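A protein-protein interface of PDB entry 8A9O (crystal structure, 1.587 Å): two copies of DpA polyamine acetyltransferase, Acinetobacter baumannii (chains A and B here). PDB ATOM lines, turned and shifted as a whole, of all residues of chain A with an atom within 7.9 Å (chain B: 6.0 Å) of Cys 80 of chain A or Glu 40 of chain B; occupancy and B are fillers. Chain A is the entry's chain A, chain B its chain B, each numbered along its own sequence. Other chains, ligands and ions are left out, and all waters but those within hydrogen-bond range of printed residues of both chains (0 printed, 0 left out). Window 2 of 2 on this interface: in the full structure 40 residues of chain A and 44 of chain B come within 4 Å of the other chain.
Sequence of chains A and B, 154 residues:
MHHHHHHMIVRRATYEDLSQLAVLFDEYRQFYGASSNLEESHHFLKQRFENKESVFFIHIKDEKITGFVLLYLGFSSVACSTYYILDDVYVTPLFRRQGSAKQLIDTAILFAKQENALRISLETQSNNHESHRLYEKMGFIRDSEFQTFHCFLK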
ATOM      1  N   PHE A  75     -13.525  32.806 -16.917  1.00  0.00           N
ATOM      2  CA  PHE A  75     -13.782  32.269 -15.590  1.00  0.00           C
ATOM      3  C   PHE A  75     -12.776  32.902 -14.622  1.00  0.00           C
ATOM      4  O   PHE A  75     -11.576  32.950 -14.919  1.00  0.00           O
ATOM      5  CB  PHE A  75     -13.615  30.733 -15.610  1.00  0.00           C
ATOM      6  CG  PHE A  75     -14.699  30.025 -16.374  1.00  0.00           C
ATOM      7  CD1 PHE A  75     -14.618  29.879 -17.753  1.00  0.00           C
ATOM      8  CD2 PHE A  75     -15.822  29.546 -15.728  1.00  0.00           C
ATOM      9  CE1 PHE A  75     -15.644  29.274 -18.462  1.00  0.00           C
ATOM     10  CE2 PHE A  75     -16.837  28.916 -16.438  1.00  0.00           C
ATOM     11  CZ  PHE A  75     -16.752  28.810 -17.802  1.00  0.00           C
ATOM     12  N   SER A  76     -13.254  33.450 -13.507  1.00  0.00           N
ATOM     13  CA  SER A  76     -12.387  34.040 -12.506  1.00  0.00           C
ATOM     14  C   SER A  76     -12.285  33.069 -11.345  1.00  0.00           C
ATOM     15  O   SER A  76     -13.257  32.927 -10.594  1.00  0.00           O
ATOM     16  CB  SER A  76     -12.971  35.351 -11.996  1.00  0.00           C
ATOM     17  OG  SER A  76     -12.211  35.844 -10.898  1.00  0.00           O
ATOM     18  N   SER A  77     -11.130  32.420 -11.179  1.00  0.00           N
ATOM     19  CA  SER A  77     -10.948  31.479 -10.070  1.00  0.00           C
ATOM     20  C   SER A  77     -11.068  32.165  -8.706  1.00  0.00           C
ATOM     21  O   SER A  77     -11.638  31.591  -7.771  1.00  0.00           O
ATOM     22  CB  SER A  77      -9.592  30.800 -10.179  1.00  0.00           C
ATOM     23  OG  SER A  77      -9.609  29.912 -11.280  1.00  0.00           O
ATOM     24  N   VAL A  78     -10.539  33.383  -8.591  1.00  0.00           N
ATOM     25  CA  VAL A  78     -10.597  34.114  -7.326  1.00  0.00           C
ATOM     26  C   VAL A  78     -12.021  34.402  -6.903  1.00  0.00           C
ATOM     27  O   VAL A  78     -12.371  34.122  -5.765  1.00  0.00           O
ATOM     28  CB  VAL A  78      -9.736  35.382  -7.397  1.00  0.00           C
ATOM     29  CG1 VAL A  78      -9.919  36.246  -6.149  1.00  0.00           C
ATOM     30  CG2 VAL A  78      -8.276  34.989  -7.579  1.00  0.00           C
ATOM     31  N   ALA A  79     -12.848  34.916  -7.812  1.00  0.00           N
ATOM     32  CA  ALA A  79     -14.239  35.243  -7.490  1.00  0.00           C
ATOM     33  C   ALA A  79     -15.190  34.050  -7.562  1.00  0.00           C
ATOM     34  O   ALA A  79     -16.336  34.161  -7.097  1.00  0.00           O
ATOM     35  CB  ALA A  79     -14.738  36.332  -8.429  1.00  0.00           C
ATOM     36  N   CYS A  80     -14.760  32.945  -8.205  1.00  0.00           N
ATOM     37  CA  CYS A  80     -15.596  31.787  -8.491  1.00  0.00           C
ATOM     38  C   CYS A  80     -16.833  32.184  -9.270  1.00  0.00           C
ATOM     39  O   CYS A  80     -17.969  31.861  -8.910  1.00  0.00           O
ATOM     40  CB  CYS A  80     -15.924  30.993  -7.238  1.00  0.00           C
ATOM     41  SG  CYS A  80     -14.532  30.016  -6.670  1.00  0.00           S
ATOM     42  N   SER A  81     -16.592  32.967 -10.311  1.00  0.00           N
ATOM     43  CA  SER A  81     -17.672  33.440 -11.145  1.00  0.00           C
ATOM     44  C   SER A  81     -17.172  33.678 -12.568  1.00  0.00           C
ATOM     45  O   SER A  81     -15.976  33.563 -12.847  1.00  0.00           O
ATOM     46  CB  SER A  81     -18.282  34.698 -10.543  1.00  0.00           C
ATOM     47  OG  SER A  81     -19.579  34.903 -11.085  1.00  0.00           O
ATOM     48  N   THR A  82     -18.092  33.962 -13.472  1.00  0.00           N
ATOM     49  CA  THR A  82     -17.721  34.190 -14.861  1.00  0.00           C
ATOM     50  C   THR A  82     -17.709  35.676 -15.200  1.00  0.00           C
ATOM     51  O   THR A  82     -18.253  36.523 -14.485  1.00  0.00           O
ATOM     52  CB  THR A  82     -18.666  33.402 -15.766  1.00  0.00           C
ATOM     53  OG1 THR A  82     -19.998  33.815 -15.461  1.00  0.00           O
ATOM     54  CG2 THR A  82     -18.542  31.911 -15.556  1.00  0.00           C
ATOM     55  N   LEU A 118     -19.231  39.242 -13.921  1.00  0.00           N
ATOM     56  CA  LEU A 118     -18.553  40.147 -12.976  1.00  0.00           C
ATOM     57  C   LEU A 118     -18.179  41.470 -13.660  1.00  0.00           C
ATOM     58  O   LEU A 118     -18.214  42.550 -13.050  1.00  0.00           O
ATOM     59  CB  LEU A 118     -17.224  39.513 -12.523  1.00  0.00           C
ATOM     60  CG  LEU A 118     -17.307  38.280 -11.683  1.00  0.00           C
ATOM     61  CD1 LEU A 118     -15.955  37.567 -11.692  1.00  0.00           C
ATOM     62  CD2 LEU A 118     -17.731  38.632 -10.244  1.00  0.00           C
ATOM     63  N   PHE B  25      -6.778  24.875  -4.398  1.00  0.00           N
ATOM     64  CA  PHE B  25      -7.487  25.899  -5.157  1.00  0.00           C
ATOM     65  C   PHE B  25      -8.057  26.942  -4.191  1.00  0.00           C
ATOM     66  O   PHE B  25      -7.927  28.131  -4.435  1.00  0.00           O
ATOM     67  CB  PHE B  25      -8.620  25.240  -5.960  1.00  0.00           C
ATOM     68  CG  PHE B  25      -9.327  26.137  -6.930  1.00  0.00           C
ATOM     69  CD1 PHE B  25      -8.683  26.601  -8.062  1.00  0.00           C
ATOM     70  CD2 PHE B  25     -10.671  26.435  -6.770  1.00  0.00           C
ATOM     71  CE1 PHE B  25      -9.358  27.376  -9.002  1.00  0.00           C
ATOM     72  CE2 PHE B  25     -11.343  27.211  -7.698  1.00  0.00           C
ATOM     73  CZ  PHE B  25     -10.691  27.673  -8.821  1.00  0.00           C
ATOM     74  N   ARG B  29      -7.148  30.970  -3.875  1.00  0.00           N
ATOM     75  CA  ARG B  29      -8.128  32.050  -3.812  1.00  0.00           C
ATOM     76  C   ARG B  29      -7.833  32.968  -2.600  1.00  0.00           C
ATOM     77  O   ARG B  29      -7.930  34.187  -2.721  1.00  0.00           O
ATOM     78  CB  ARG B  29      -9.536  31.460  -3.714  1.00  0.00           C
ATOM     79  CG  ARG B  29      -9.953  30.674  -4.979  1.00  0.00           C
ATOM     80  CD  ARG B  29     -11.404  30.251  -4.882  1.00  0.00           C
ATOM     81  NE  ARG B  29     -12.268  31.425  -4.740  1.00  0.00           N
ATOM     82  CZ  ARG B  29     -13.298  31.509  -3.906  1.00  0.00           C
ATOM     83  NH1 ARG B  29     -13.643  30.464  -3.160  1.00  0.00           N
ATOM     84  NH2 ARG B  29     -14.006  32.631  -3.826  1.00  0.00           N
ATOM     85  N   SER B  35     -12.239  34.854   0.905  1.00  0.00           N
ATOM     86  CA  SER B  35     -12.427  34.146   2.163  1.00  0.00           C
ATOM     87  C   SER B  35     -12.492  32.656   1.848  1.00  0.00           C
ATOM     88  O   SER B  35     -13.101  32.279   0.845  1.00  0.00           O
ATOM     89  CB  SER B  35     -13.740  34.560   2.825  1.00  0.00           C
ATOM     90  OG  SER B  35     -13.708  35.916   3.236  1.00  0.00           O
ATOM     91  N   SER B  36     -11.925  31.811   2.711  1.00  0.00           N
ATOM     92  CA  SER B  36     -11.963  30.366   2.515  1.00  0.00           C
ATOM     93  C   SER B  36     -13.392  29.846   2.476  1.00  0.00           C
ATOM     94  O   SER B  36     -14.198  30.143   3.365  1.00  0.00           O
ATOM     95  CB  SER B  36     -11.177  29.647   3.608  1.00  0.00           C
ATOM     96  OG  SER B  36     -11.195  28.237   3.433  1.00  0.00           O
ATOM     97  N   ASN B  37     -13.708  29.069   1.445  1.00  0.00           N
ATOM     98  CA  ASN B  37     -15.033  28.483   1.303  1.00  0.00           C
ATOM     99  C   ASN B  37     -14.840  27.246   0.445  1.00  0.00           C
ATOM    100  O   ASN B  37     -14.857  27.336  -0.775  1.00  0.00           O
ATOM    101  CB  ASN B  37     -15.988  29.478   0.654  1.00  0.00           C
ATOM    102  CG  ASN B  37     -17.420  29.024   0.678  1.00  0.00           C
ATOM    103  OD1 ASN B  37     -17.700  27.832   0.625  1.00  0.00           O
ATOM    104  ND2 ASN B  37     -18.355  29.974   0.722  1.00  0.00           N
ATOM    105  N   LEU B  38     -14.582  26.106   1.089  1.00  0.00           N
ATOM    106  CA  LEU B  38     -14.307  24.876   0.375  1.00  0.00           C
ATOM    107  C   LEU B  38     -15.446  24.433  -0.527  1.00  0.00           C
ATOM    108  O   LEU B  38     -15.182  23.956  -1.616  1.00  0.00           O
ATOM    109  CB  LEU B  38     -13.881  23.750   1.304  1.00  0.00           C
ATOM    110  CG  LEU B  38     -12.487  23.899   1.900  1.00  0.00           C
ATOM    111  CD1 LEU B  38     -12.298  22.936   3.072  1.00  0.00           C
ATOM    112  CD2 LEU B  38     -11.398  23.658   0.848  1.00  0.00           C
ATOM    113  N   GLU B  39     -16.699  24.627  -0.121  1.00  0.00           N
ATOM    114  CA  GLU B  39     -17.834  24.248  -0.945  1.00  0.00           C
ATOM    115  C   GLU B  39     -17.843  25.045  -2.270  1.00  0.00           C
ATOM    116  O   GLU B  39     -18.022  24.472  -3.344  1.00  0.00           O
ATOM    117  CB  GLU B  39     -19.151  24.453  -0.176  1.00  0.00           C
ATOM    118  CG  GLU B  39     -20.378  24.056  -0.974  1.00  0.00           C
ATOM    119  N   GLU B  40     -17.669  26.368  -2.174  1.00  0.00           N
ATOM    120  CA  GLU B  40     -17.664  27.276  -3.301  1.00  0.00           C
ATOM    121  C   GLU B  40     -16.442  26.967  -4.187  1.00  0.00           C
ATOM    122  O   GLU B  40     -16.590  26.844  -5.396  1.00  0.00           O
ATOM    123  CB  GLU B  40     -17.586  28.708  -2.761  1.00  0.00           C
ATOM    124  CG  GLU B  40     -17.432  29.769  -3.822  1.00  0.00           C
ATOM    125  CD  GLU B  40     -17.235  31.161  -3.261  1.00  0.00           C
ATOM    126  OE1 GLU B  40     -16.407  31.332  -2.330  1.00  0.00           O
ATOM    127  OE2 GLU B  40     -17.909  32.088  -3.768  1.00  0.00           O
ATOM    128  N   SER B  41     -15.258  26.804  -3.575  1.00  0.00           N
ATOM    129  CA  SER B  41     -14.040  26.510  -4.318  1.00  0.00           C
ATOM    130  C   SER B  41     -14.143  25.189  -5.069  1.00  0.00           C
ATOM    131  O   SER B  41     -13.821  25.140  -6.253  1.00  0.00           O
ATOM    132  CB  SER B  41     -12.818  26.532  -3.405  1.00  0.00           C
ATOM    133  OG  SER B  41     -12.660  27.817  -2.828  1.00  0.00           O
ATOM    134  N   HIS B  42     -14.645  24.133  -4.415  1.00  0.00           N
ATOM    135  CA  HIS B  42     -14.784  22.831  -5.059  1.00  0.00           C
ATOM    136  C   HIS B  42     -15.797  22.872  -6.183  1.00  0.00           C
ATOM    137  O   HIS B  42     -15.549  22.305  -7.246  1.00  0.00           O
ATOM    138  CB  HIS B  42     -15.166  21.760  -4.036  1.00  0.00           C
ATOM    139  CG  HIS B  42     -15.328  20.382  -4.612  1.00  0.00           C
ATOM    140  ND1 HIS B  42     -14.309  19.451  -4.519  1.00  0.00           N
ATOM    141  CD2 HIS B  42     -16.399  19.788  -5.193  1.00  0.00           C
ATOM    142  CE1 HIS B  42     -14.770  18.338  -5.075  1.00  0.00           C
ATOM    143  NE2 HIS B  42     -16.020  18.473  -5.473  1.00  0.00           N
ATOM    144  N   HIS B  43     -16.936  23.559  -5.986  1.00  0.00           N
ATOM    145  CA  HIS B  43     -17.956  23.664  -7.017  1.00  0.00           C
ATOM    146  C   HIS B  43     -17.395  24.313  -8.291  1.00  0.00           C
ATOM    147  O   HIS B  43     -17.604  23.804  -9.387  1.00  0.00           O
ATOM    148  CB  HIS B  43     -19.151  24.472  -6.498  1.00  0.00           C
ATOM    149  CG  HIS B  43     -20.253  24.595  -7.495  1.00  0.00           C
ATOM    150  ND1 HIS B  43     -21.281  23.649  -7.574  1.00  0.00           N
ATOM    151  CD2 HIS B  43     -20.470  25.554  -8.421  1.00  0.00           C
ATOM    152  CE1 HIS B  43     -22.079  24.073  -8.538  1.00  0.00           C
ATOM    153  NE2 HIS B  43     -21.633  25.210  -9.081  1.00  0.00           N
ATOM    154  N   PHE B  44     -16.648  25.403  -8.128  1.00  0.00           N
ATOM    155  CA  PHE B  44     -16.101  26.133  -9.268  1.00  0.00           C
ATOM    156  C   PHE B  44     -14.956  25.392  -9.914  1.00  0.00           C
ATOM    157  O   PHE B  44     -14.844  25.379 -11.138  1.00  0.00           O
ATOM    158  CB  PHE B  44     -15.680  27.529  -8.847  1.00  0.00           C
ATOM    159  CG  PHE B  44     -15.497  28.439 -10.027  1.00  0.00           C
ATOM    160  CD1 PHE B  44     -16.589  28.884 -10.752  1.00  0.00           C
ATOM    161  CD2 PHE B  44     -14.239  28.858 -10.401  1.00  0.00           C
ATOM    162  CE1 PHE B  44     -16.417  29.726 -11.835  1.00  0.00           C
ATOM    163  CE2 PHE B  44     -14.074  29.706 -11.477  1.00  0.00           C
ATOM    164  CZ  PHE B  44     -15.160  30.133 -12.188  1.00  0.00           C
ATOM    165  N   LEU B  45     -14.139  24.707  -9.107  1.00  0.00           N
ATOM    166  CA  LEU B  45     -13.052  23.880  -9.626  1.00  0.00           C
ATOM    167  C   LEU B  45     -13.653  22.754 -10.504  1.00  0.00           C
ATOM    168  O   LEU B  45     -13.156  22.489 -11.595  1.00  0.00           O
ATOM    169  CB  LEU B  45     -12.271  23.276  -8.455  1.00  0.00           C
ATOM    170  CG  LEU B  45     -11.216  22.240  -8.821  1.00  0.00           C
ATOM    171  CD1 LEU B  45     -10.061  22.923  -9.495  1.00  0.00           C
ATOM    172  CD2 LEU B  45     -10.742  21.478  -7.609  1.00  0.00           C
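O of Val 78 of chain A is in hydrogen-bond range of NE of Arg 29 of chain B (2.9 Å). NE of Arg 29 of chain B sits at hydrogen-bond distance from O of Ser 77 of chain A. The side-chain sulfur of Cys 80 of chain A is in hydrogen-bond range of the guanidinium group of Arg 29 of chain B (3.3 Å).
No position is printed for both chains.
Of the 13 printed residues of chain B, 4 touch a printed residue of chain A. Along chain B the printed residues that touch a printed residue of chain A span positions 25 to 44. Of the 9 printed residues of chain A, 6 touch a printed residue of chain B. Hydrophobic or aromatic side chains of chain A within 4 Å of the printed part of chain B: Phe 75. Among the printed residues, no Asp or Glu carboxylate lies within 4 Å of a Lys or Arg side-chain nitrogen of the other chain.
Of the printed residues of chain B, Cys 80 of chain A touches Arg 29 (3.3 Å), Glu 40 (3.9 Å) and Phe 44 (3.5 Å). Of the printed residues of chain A, Glu 40 of chain B touches Cys 80 (3.9 Å). Of the printed residues of chain B, Ser 77 of chain A touches Phe 25 (3.4 Å), Arg 29 (3.1 Å) and Phe 44 (3.9 Å). Of the printed residues of chain B, Ser 76 of chain A touches Phe 44 (3.4 Å). Of the printed residues of chain B, Ser 81 of chain A touches Phe 44. Of the printed residues of chain A, Phe 25 of chain B touches Ser 77 (3.4 Å). Of the printed residues of chain A, Phe 44 of chain B touches Phe 75 (3.6 Å), Ser 76 (3.4 Å), Ser 77 (3.9 Å), Cys 80 (3.5 Å) and Ser 81 (3.6 Å). The nearest residue of chain A that does not touch Glu 40 of chain B is Ala 79 of chain A (4.2 Å). The nearest printed residue of chain B that does not touch Ser 76 of chain A is Phe 25 of chain B (6.1 Å).
Among the printed residues, pairs that only touch across the chains: Ser 77 of chain A with Phe 25 of chain B (3.4 Å), Ser 76 of chain A with Phe 44 of chain B (3.4 Å), Cys 80 of chain A with Phe 44 of chain B (3.5 Å), Ser 81 of chain A with Phe 44 of chain B (3.6 Å), Phe 75 of chain A with Phe 44 of chain B (3.6 Å), Ser 77 of chain A with Phe 44 of chain B (3.9 Å) and Cys 80 of chain A with Glu 40 of chain B (3.9 Å).
The guanidinium group (NH1) of Arg 29 of chain B sits at hydrogen-bond distance from the side-chain hydroxyl (OG) of Ser 41 of chain B (2.8 Å). The guanidinium group of Arg 29 of chain B lies within salt-bridge range of the side-chain carboxylate of Glu 40 of chain B (3.0 Å). The side-chain amide oxygen (OD1) of Asn 37 of chain B lies within hydrogen-bond range of the backbone NH (N) of Glu 40 of chain B, at 3.2 Å. SG of Cys 80 of chain A is in hydrogen-bond range of O of Ser 77 of chain A (3.5 Å). The backbone NH (N) of Ala 79 of chain A lies within hydrogen-bond range of the side-chain hydroxyl (OG) of Ser 76 of chain A, at 3.3 Å. The backbone NH of Ser 76 of chain A lies within hydrogen-bond range of the backbone carbonyl oxygen of Ser 81 of chain A, 2.8 Å away.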
